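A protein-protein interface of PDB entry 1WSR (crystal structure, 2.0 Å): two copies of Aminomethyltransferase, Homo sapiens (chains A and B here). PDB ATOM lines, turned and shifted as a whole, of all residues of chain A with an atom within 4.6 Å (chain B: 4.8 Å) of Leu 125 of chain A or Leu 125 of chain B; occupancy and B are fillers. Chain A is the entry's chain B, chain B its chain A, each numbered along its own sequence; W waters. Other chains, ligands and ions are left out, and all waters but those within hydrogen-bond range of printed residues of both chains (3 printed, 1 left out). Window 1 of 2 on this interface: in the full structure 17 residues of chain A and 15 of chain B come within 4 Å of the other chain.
The side-chain carboxylate (OE1) of Glu 122 of chain B sits close to the indole nitrogen (NE1) of Trp 121 of chain B (3.5 Å).
Among the printed residues, merely in contact across the chains: Trp 121 of chain A with Trp 121 of chain B (3.96 Å), Trp 121 of chain A with Glu 122 of chain B (3.8 Å), Trp 121 of chain A with Leu 125 of chain B (3.9 Å), Glu 122 of chain A with Trp 121 of chain B (3.7 Å), Glu 122 of chain A with Glu 122 of chain B (3.8 Å), Leu 125 of chain A with Trp 121 of chain B (3.95 Å), Leu 125 of chain A with Leu 125 of chain B (3.9 Å) and Val 146 of chain A with Gln 129 of chain B (3.8 Å).
Of chain B, only Trp 121 and Leu 125 come within 4 Å of Leu 125 of chain A. Of chain A, only Trp 121 and Leu 125 come within 4 Å of Leu 125 of chain B. Of the printed residues of chain A, Glu 122 of chain B touches Trp 121 and Glu 122. Printed residues of chain B within 4 Å of Glu 122 of chain A: Trp 121 and Glu 122. Printed residues of chain B within 4 Å of Trp 121 of chain A: Trp 121, Glu 122 and Leu 125. Of the printed residues of chain A, Trp 121 of chain B touches Trp 121 (3.96 Å), Glu 122 (3.7 Å) and Leu 125 (3.95 Å). Ala 126 of chain B touches none of the printed residues of chain A. The nearest printed residue of chain B that does not touch Leu 125 of chain A is Val 146 of chain B (5.5 Å). The nearest printed residue of chain B that does not touch Trp 121 of chain A is Ala 126 of chain B (4.3 Å).
Of the 13 printed residues of chain B, 4 touch a printed residue of chain A. Printed residues of chain B that touch a printed residue of chain A: Trp 121, Glu 122, Leu 125 and Gln 129. Hydrophobic or aromatic side chains of chain B within 4 Å of the printed part of chain A: Trp 121 and Leu 125. Hydrophobic or aromatic side chains of chain A that line the printed part of chain B: Trp 121, Leu 125 and Val 146.
Trp 121 of chain A touches Glu 122 of chain B, and with the chains exchanged Glu 122 of chain A touches Trp 121 of chain B. Glu 122 of chain A touches its own counterpart, Glu 122 of chain B. Leu 125 of chain B touches its own counterpart, Leu 125 of chain A. Val 146 of chain A touches Gln 129 of chain B, but with the chains exchanged Gln 129 of chain A does not touch Val 146 of chain B (4.4 Å). Of the 8 pairs that touch across the chains among the printed residues, 7 have their exchanged pair printed and touching as well.
Water W2 bridges the backbone carbonyl oxygen of Leu 144 of chain B (2.7 Å) and the backbone carbonyl oxygen of Val 146 of chain A (2.9 Å). Water W1 lies within hydrogen-bond range of O of Val 146 of chain A and O of Leu 144 of chain B. Water W3 bridges the backbone NH (N) of Val 146 of chain A (3.1 Å) and the backbone NH (N) of Val 146 of chain B (3.2 Å).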
ATOM      1  N   LEU A  57     -28.010 -28.099 -30.507  1.00  0.00           N
ATOM      2  CA  LEU A  57     -27.658 -27.274 -29.359  1.00  0.00           C
ATOM      3  C   LEU A  57     -28.308 -27.841 -28.100  1.00  0.00           C
ATOM      4  O   LEU A  57     -29.523 -28.041 -28.056  1.00  0.00           O
ATOM      5  CB  LEU A  57     -28.133 -25.832 -29.563  1.00  0.00           C
ATOM      6  CG  LEU A  57     -27.891 -24.894 -28.372  1.00  0.00           C
ATOM      7  CD1 LEU A  57     -26.392 -24.712 -28.163  1.00  0.00           C
ATOM      8  CD2 LEU A  57     -28.557 -23.549 -28.623  1.00  0.00           C
ATOM      9  N   CYS A 120     -29.943 -23.384 -36.038  1.00  0.00           N
ATOM     10  CA  CYS A 120     -30.393 -22.150 -35.393  1.00  0.00           C
ATOM     11  C   CYS A 120     -29.698 -21.910 -34.056  1.00  0.00           C
ATOM     12  O   CYS A 120     -30.186 -21.123 -33.241  1.00  0.00           O
ATOM     13  CB  CYS A 120     -31.901 -22.198 -35.129  1.00  0.00           C
ATOM     14  SG  CYS A 120     -32.946 -22.473 -36.570  1.00  0.00           S
ATOM     15  N   TRP A 121     -28.565 -22.559 -33.817  1.00  0.00           N
ATOM     16  CA  TRP A 121     -27.915 -22.384 -32.524  1.00  0.00           C
ATOM     17  C   TRP A 121     -27.522 -20.946 -32.203  1.00  0.00           C
ATOM     18  O   TRP A 121     -27.720 -20.496 -31.076  1.00  0.00           O
ATOM     19  CB  TRP A 121     -26.709 -23.327 -32.370  1.00  0.00           C
ATOM     20  CG  TRP A 121     -25.422 -22.892 -33.007  1.00  0.00           C
ATOM     21  CD1 TRP A 121     -24.950 -23.245 -34.241  1.00  0.00           C
ATOM     22  CD2 TRP A 121     -24.408 -22.073 -32.410  1.00  0.00           C
ATOM     23  NE1 TRP A 121     -23.701 -22.703 -34.446  1.00  0.00           N
ATOM     24  CE2 TRP A 121     -23.345 -21.978 -33.338  1.00  0.00           C
ATOM     25  CE3 TRP A 121     -24.294 -21.412 -31.179  1.00  0.00           C
ATOM     26  CZ2 TRP A 121     -22.180 -21.245 -33.073  1.00  0.00           C
ATOM     27  CZ3 TRP A 121     -23.134 -20.682 -30.913  1.00  0.00           C
ATOM     28  CH2 TRP A 121     -22.091 -20.607 -31.861  1.00  0.00           C
ATOM     29  N   GLU A 122     -26.989 -20.216 -33.177  1.00  0.00           N
ATOM     30  CA  GLU A 122     -26.593 -18.832 -32.925  1.00  0.00           C
ATOM     31  C   GLU A 122     -27.803 -17.992 -32.525  1.00  0.00           C
ATOM     32  O   GLU A 122     -27.741 -17.215 -31.572  1.00  0.00           O
ATOM     33  CB  GLU A 122     -25.931 -18.223 -34.162  1.00  0.00           C
ATOM     34  CG  GLU A 122     -24.718 -19.001 -34.649  1.00  0.00           C
ATOM     35  CD  GLU A 122     -25.019 -19.843 -35.872  1.00  0.00           C
ATOM     36  OE1 GLU A 122     -26.063 -20.540 -35.886  1.00  0.00           O
ATOM     37  OE2 GLU A 122     -24.204 -19.806 -36.818  1.00  0.00           O
ATOM     38  N   LYS A 123     -28.897 -18.161 -33.263  1.00  0.00           N
ATOM     39  CA  LYS A 123     -30.139 -17.441 -33.002  1.00  0.00           C
ATOM     40  C   LYS A 123     -30.740 -17.816 -31.648  1.00  0.00           C
ATOM     41  O   LYS A 123     -31.039 -16.946 -30.824  1.00  0.00           O
ATOM     42  CB  LYS A 123     -31.168 -17.756 -34.097  1.00  0.00           C
ATOM     43  CG  LYS A 123     -32.518 -17.071 -33.905  1.00  0.00           C
ATOM     44  CD  LYS A 123     -33.672 -17.838 -34.570  1.00  0.00           C
ATOM     45  CE  LYS A 123     -33.503 -17.973 -36.075  1.00  0.00           C
ATOM     46  NZ  LYS A 123     -34.713 -18.578 -36.716  1.00  0.00           N
ATOM     47  N   ASP A 124     -30.928 -19.116 -31.431  1.00  0.00           N
ATOM     48  CA  ASP A 124     -31.524 -19.612 -30.193  1.00  0.00           C
ATOM     49  C   ASP A 124     -30.690 -19.302 -28.956  1.00  0.00           C
ATOM     50  O   ASP A 124     -31.231 -18.912 -27.922  1.00  0.00           O
ATOM     51  CB  ASP A 124     -31.759 -21.124 -30.274  1.00  0.00           C
ATOM     52  CG  ASP A 124     -32.733 -21.515 -31.378  1.00  0.00           C
ATOM     53  OD1 ASP A 124     -33.372 -20.622 -31.980  1.00  0.00           O
ATOM     54  OD2 ASP A 124     -32.865 -22.728 -31.636  1.00  0.00           O
ATOM     55  N   LEU A 125     -29.375 -19.480 -29.048  1.00  0.00           N
ATOM     56  CA  LEU A 125     -28.524 -19.200 -27.900  1.00  0.00           C
ATOM     57  C   LEU A 125     -28.598 -17.718 -27.530  1.00  0.00           C
ATOM     58  O   LEU A 125     -28.686 -17.365 -26.352  1.00  0.00           O
ATOM     59  CB  LEU A 125     -27.072 -19.600 -28.189  1.00  0.00           C
ATOM     60  CG  LEU A 125     -26.092 -19.391 -27.028  1.00  0.00           C
ATOM     61  CD1 LEU A 125     -26.616 -20.098 -25.778  1.00  0.00           C
ATOM     62  CD2 LEU A 125     -24.715 -19.932 -27.406  1.00  0.00           C
ATOM     63  N   ALA A 126     -28.570 -16.850 -28.536  1.00  0.00           N
ATOM     64  CA  ALA A 126     -28.642 -15.413 -28.290  1.00  0.00           C
ATOM     65  C   ALA A 126     -29.979 -15.062 -27.647  1.00  0.00           C
ATOM     66  O   ALA A 126     -30.044 -14.263 -26.711  1.00  0.00           O
ATOM     67  CB  ALA A 126     -28.472 -14.648 -29.599  1.00  0.00           C
ATOM     68  N   LEU A 127     -31.046 -15.670 -28.152  1.00  0.00           N
ATOM     69  CA  LEU A 127     -32.390 -15.429 -27.639  1.00  0.00           C
ATOM     70  C   LEU A 127     -32.489 -15.754 -26.147  1.00  0.00           C
ATOM     71  O   LEU A 127     -32.971 -14.947 -25.350  1.00  0.00           O
ATOM     72  CB  LEU A 127     -33.397 -16.285 -28.408  1.00  0.00           C
ATOM     73  CG  LEU A 127     -34.867 -16.088 -28.045  1.00  0.00           C
ATOM     74  CD1 LEU A 127     -35.345 -14.742 -28.577  1.00  0.00           C
ATOM     75  CD2 LEU A 127     -35.692 -17.217 -28.639  1.00  0.00           C
ATOM     76  N   MET A 128     -32.037 -16.948 -25.781  1.00  0.00           N
ATOM     77  CA  MET A 128     -32.078 -17.386 -24.393  1.00  0.00           C
ATOM     78  C   MET A 128     -31.130 -16.591 -23.501  1.00  0.00           C
ATOM     79  O   MET A 128     -31.505 -16.185 -22.399  1.00  0.00           O
ATOM     80  CB  MET A 128     -31.756 -18.883 -24.300  1.00  0.00           C
ATOM     81  CG  MET A 128     -32.822 -19.773 -24.940  1.00  0.00           C
ATOM     82  SD  MET A 128     -32.583 -21.544 -24.653  1.00  0.00           S
ATOM     83  CE  MET A 128     -31.477 -21.960 -25.983  1.00  0.00           C
ATOM     84  N   GLN A 129     -29.910 -16.361 -23.977  1.00  0.00           N
ATOM     85  CA  GLN A 129     -28.926 -15.611 -23.201  1.00  0.00           C
ATOM     86  C   GLN A 129     -29.401 -14.183 -22.931  1.00  0.00           C
ATOM     87  O   GLN A 129     -29.221 -13.663 -21.829  1.00  0.00           O
ATOM     88  CB  GLN A 129     -27.576 -15.586 -23.930  1.00  0.00           C
ATOM     89  CG  GLN A 129     -26.470 -14.862 -23.167  1.00  0.00           C
ATOM     90  CD  GLN A 129     -26.104 -15.548 -21.860  1.00  0.00           C
ATOM     91  OE1 GLN A 129     -25.447 -16.592 -21.851  1.00  0.00           O
ATOM     92  NE2 GLN A 129     -26.538 -14.966 -20.743  1.00  0.00           N
ATOM     93  N   LEU A 144     -27.840 -19.773 -17.508  1.00  0.00           N
ATOM     94  CA  LEU A 144     -27.814 -20.650 -18.666  1.00  0.00           C
ATOM     95  C   LEU A 144     -26.429 -21.244 -18.872  1.00  0.00           C
ATOM     96  O   LEU A 144     -25.418 -20.561 -18.694  1.00  0.00           O
ATOM     97  CB  LEU A 144     -28.233 -19.861 -19.912  1.00  0.00           C
ATOM     98  CG  LEU A 144     -28.365 -20.565 -21.264  1.00  0.00           C
ATOM     99  CD1 LEU A 144     -29.076 -19.631 -22.232  1.00  0.00           C
ATOM    100  CD2 LEU A 144     -26.998 -20.954 -21.809  1.00  0.00           C
ATOM    101  N   VAL A 146     -24.243 -23.890 -21.651  1.00  0.00           N
ATOM    102  CA  VAL A 146     -24.264 -24.619 -22.908  1.00  0.00           C
ATOM    103  C   VAL A 146     -23.573 -25.943 -22.628  1.00  0.00           C
ATOM    104  O   VAL A 146     -22.414 -25.967 -22.216  1.00  0.00           O
ATOM    105  CB  VAL A 146     -23.505 -23.870 -24.022  1.00  0.00           C
ATOM    106  CG1 VAL A 146     -23.453 -24.726 -25.285  1.00  0.00           C
ATOM    107  CG2 VAL A 146     -24.192 -22.548 -24.315  1.00  0.00           C
ATOM    108  N   LEU B  57     -17.859 -10.933 -26.100  1.00  0.00           N
ATOM    109  CA  LEU B  57     -17.995 -12.300 -25.604  1.00  0.00           C
ATOM    110  C   LEU B  57     -17.064 -12.531 -24.417  1.00  0.00           C
ATOM    111  O   LEU B  57     -15.857 -12.309 -24.518  1.00  0.00           O
ATOM    112  CB  LEU B  57     -17.653 -13.312 -26.697  1.00  0.00           C
ATOM    113  CG  LEU B  57     -17.648 -14.779 -26.242  1.00  0.00           C
ATOM    114  CD1 LEU B  57     -19.050 -15.188 -25.812  1.00  0.00           C
ATOM    115  CD2 LEU B  57     -17.162 -15.676 -27.376  1.00  0.00           C
ATOM    116  N   CYS B 120     -17.486 -11.310 -33.520  1.00  0.00           N
ATOM    117  CA  CYS B 120     -16.893 -12.612 -33.828  1.00  0.00           C
ATOM    118  C   CYS B 120     -17.302 -13.668 -32.808  1.00  0.00           C
ATOM    119  O   CYS B 120     -16.689 -14.735 -32.744  1.00  0.00           O
ATOM    120  CB  CYS B 120     -15.361 -12.520 -33.824  1.00  0.00           C
ATOM    121  SG  CYS B 120     -14.619 -11.487 -35.103  1.00  0.00           S
ATOM    122  N   TRP B 121     -18.337 -13.396 -32.018  1.00  0.00           N
ATOM    123  CA  TRP B 121     -18.713 -14.352 -30.984  1.00  0.00           C
ATOM    124  C   TRP B 121     -19.117 -15.741 -31.476  1.00  0.00           C
ATOM    125  O   TRP B 121     -18.772 -16.736 -30.846  1.00  0.00           O
ATOM    126  CB  TRP B 121     -19.801 -13.771 -30.066  1.00  0.00           C
ATOM    127  CG  TRP B 121     -21.206 -13.883 -30.565  1.00  0.00           C
ATOM    128  CD1 TRP B 121     -21.884 -12.982 -31.337  1.00  0.00           C
ATOM    129  CD2 TRP B 121     -22.120 -14.951 -30.295  1.00  0.00           C
ATOM    130  NE1 TRP B 121     -23.170 -13.422 -31.560  1.00  0.00           N
ATOM    131  CE2 TRP B 121     -23.340 -14.628 -30.932  1.00  0.00           C
ATOM    132  CE3 TRP B 121     -22.027 -16.149 -29.575  1.00  0.00           C
ATOM    133  CZ2 TRP B 121     -24.462 -15.463 -30.870  1.00  0.00           C
ATOM    134  CZ3 TRP B 121     -23.143 -16.980 -29.513  1.00  0.00           C
ATOM    135  CH2 TRP B 121     -24.346 -16.630 -30.159  1.00  0.00           C
ATOM    136  N   GLU B 122     -19.831 -15.820 -32.593  1.00  0.00           N
ATOM    137  CA  GLU B 122     -20.245 -17.122 -33.108  1.00  0.00           C
ATOM    138  C   GLU B 122     -19.017 -17.920 -33.542  1.00  0.00           C
ATOM    139  O   GLU B 122     -18.869 -19.092 -33.190  1.00  0.00           O
ATOM    140  CB  GLU B 122     -21.205 -16.957 -34.293  1.00  0.00           C
ATOM    141  CG  GLU B 122     -22.418 -16.097 -33.978  1.00  0.00           C
ATOM    142  CD  GLU B 122     -22.273 -14.664 -34.475  1.00  0.00           C
ATOM    143  OE1 GLU B 122     -21.169 -14.079 -34.347  1.00  0.00           O
ATOM    144  OE2 GLU B 122     -23.276 -14.118 -34.986  1.00  0.00           O
ATOM    145  N   LYS B 123     -18.139 -17.266 -34.296  1.00  0.00           N
ATOM    146  CA  LYS B 123     -16.907 -17.877 -34.789  1.00  0.00           C
ATOM    147  C   LYS B 123     -15.987 -18.308 -33.646  1.00  0.00           C
ATOM    148  O   LYS B 123     -15.513 -19.443 -33.611  1.00  0.00           O
ATOM    149  CB  LYS B 123     -16.150 -16.881 -35.679  1.00  0.00           C
ATOM    150  CG  LYS B 123     -14.807 -17.387 -36.189  1.00  0.00           C
ATOM    151  CD  LYS B 123     -13.810 -16.248 -36.427  1.00  0.00           C
ATOM    152  CE  LYS B 123     -14.308 -15.246 -37.455  1.00  0.00           C
ATOM    153  NZ  LYS B 123     -13.316 -14.151 -37.704  1.00  0.00           N
ATOM    154  N   ASP B 124     -15.725 -17.386 -32.723  1.00  0.00           N
ATOM    155  CA  ASP B 124     -14.839 -17.662 -31.592  1.00  0.00           C
ATOM    156  C   ASP B 124     -15.375 -18.736 -30.659  1.00  0.00           C
ATOM    157  O   ASP B 124     -14.632 -19.614 -30.223  1.00  0.00           O
ATOM    158  CB  ASP B 124     -14.581 -16.391 -30.776  1.00  0.00           C
ATOM    159  CG  ASP B 124     -13.832 -15.325 -31.560  1.00  0.00           C
ATOM    160  OD1 ASP B 124     -13.352 -15.608 -32.683  1.00  0.00           O
ATOM    161  OD2 ASP B 124     -13.718 -14.198 -31.040  1.00  0.00           O
ATOM    162  N   LEU B 125     -16.659 -18.661 -30.330  1.00  0.00           N
ATOM    163  CA  LEU B 125     -17.233 -19.658 -29.440  1.00  0.00           C
ATOM    164  C   LEU B 125     -17.149 -21.050 -30.065  1.00  0.00           C
ATOM    165  O   LEU B 125     -16.760 -22.007 -29.402  1.00  0.00           O
ATOM    166  CB  LEU B 125     -18.686 -19.314 -29.102  1.00  0.00           C
ATOM    167  CG  LEU B 125     -19.403 -20.314 -28.190  1.00  0.00           C
ATOM    168  CD1 LEU B 125     -18.604 -20.519 -26.907  1.00  0.00           C
ATOM    169  CD2 LEU B 125     -20.809 -19.803 -27.881  1.00  0.00           C
ATOM    170  N   ALA B 126     -17.500 -21.156 -31.345  1.00  0.00           N
ATOM    171  CA  ALA B 126     -17.453 -22.441 -32.041  1.00  0.00           C
ATOM    172  C   ALA B 126     -16.024 -22.978 -32.076  1.00  0.00           C
ATOM    173  O   ALA B 126     -15.792 -24.176 -31.899  1.00  0.00           O
ATOM    174  CB  ALA B 126     -17.986 -22.288 -33.467  1.00  0.00           C
ATOM    175  N   LEU B 127     -15.071 -22.083 -32.304  1.00  0.00           N
ATOM    176  CA  LEU B 127     -13.664 -22.463 -32.369  1.00  0.00           C
ATOM    177  C   LEU B 127     -13.207 -23.063 -31.047  1.00  0.00           C
ATOM    178  O   LEU B 127     -12.550 -24.110 -31.017  1.00  0.00           O
ATOM    179  CB  LEU B 127     -12.801 -21.240 -32.692  1.00  0.00           C
ATOM    180  CG  LEU B 127     -11.287 -21.473 -32.720  1.00  0.00           C
ATOM    181  CD1 LEU B 127     -10.912 -22.219 -33.990  1.00  0.00           C
ATOM    182  CD2 LEU B 127     -10.556 -20.140 -32.662  1.00  0.00           C
ATOM    183  N   MET B 128     -13.548 -22.395 -29.952  1.00  0.00           N
ATOM    184  CA  MET B 128     -13.157 -22.884 -28.639  1.00  0.00           C
ATOM    185  C   MET B 128     -13.902 -24.169 -28.292  1.00  0.00           C
ATOM    186  O   MET B 128     -13.318 -25.087 -27.716  1.00  0.00           O
ATOM    187  CB  MET B 128     -13.390 -21.802 -27.580  1.00  0.00           C
ATOM    188  CG  MET B 128     -12.466 -20.598 -27.766  1.00  0.00           C
ATOM    189  SD  MET B 128     -12.532 -19.396 -26.424  1.00  0.00           S
ATOM    190  CE  MET B 128     -14.008 -18.460 -26.881  1.00  0.00           C
ATOM    191  N   GLN B 129     -15.182 -24.238 -28.654  1.00  0.00           N
ATOM    192  CA  GLN B 129     -15.980 -25.436 -28.396  1.00  0.00           C
ATOM    193  C   GLN B 129     -15.384 -26.630 -29.137  1.00  0.00           C
ATOM    194  O   GLN B 129     -15.276 -27.725 -28.583  1.00  0.00           O
ATOM    195  CB  GLN B 129     -17.420 -25.250 -28.874  1.00  0.00           C
ATOM    196  CG  GLN B 129     -18.239 -24.231 -28.111  1.00  0.00           C
ATOM    197  CD  GLN B 129     -19.666 -24.166 -28.630  1.00  0.00           C
ATOM    198  OE1 GLN B 129     -19.893 -24.121 -29.840  1.00  0.00           O
ATOM    199  NE2 GLN B 129     -20.633 -24.156 -27.718  1.00  0.00           N
ATOM    200  N   LEU B 144     -15.575 -25.212 -21.011  1.00  0.00           N
ATOM    201  CA  LEU B 144     -15.776 -23.799 -21.267  1.00  0.00           C
ATOM    202  C   LEU B 144     -17.135 -23.327 -20.766  1.00  0.00           C
ATOM    203  O   LEU B 144     -18.113 -24.070 -20.803  1.00  0.00           O
ATOM    204  CB  LEU B 144     -15.641 -23.526 -22.770  1.00  0.00           C
ATOM    205  CG  LEU B 144     -16.094 -22.166 -23.311  1.00  0.00           C
ATOM    206  CD1 LEU B 144     -15.340 -21.849 -24.592  1.00  0.00           C
ATOM    207  CD2 LEU B 144     -17.599 -22.181 -23.561  1.00  0.00           C
ATOM    208  N   VAL B 146     -19.785 -19.839 -20.932  1.00  0.00           N
ATOM    209  CA  VAL B 146     -20.058 -18.526 -21.495  1.00  0.00           C
ATOM    210  C   VAL B 146     -20.618 -17.715 -20.332  1.00  0.00           C
ATOM    211  O   VAL B 146     -21.588 -18.129 -19.698  1.00  0.00           O
ATOM    212  CB  VAL B 146     -21.110 -18.591 -22.618  1.00  0.00           C
ATOM    213  CG1 VAL B 146     -21.347 -17.193 -23.179  1.00  0.00           C
ATOM    214  CG2 VAL B 146     -20.645 -19.537 -23.715  1.00  0.00           C
HETATM  215  O   HOH W   1     -20.060 -26.789 -21.231  1.00  0.00           O
HETATM  216  O   HOH W   2     -20.125 -24.284 -22.522  1.00  0.00           O
HETATM  217  O   HOH W   3     -21.957 -22.103 -20.619  1.00  0.00           O
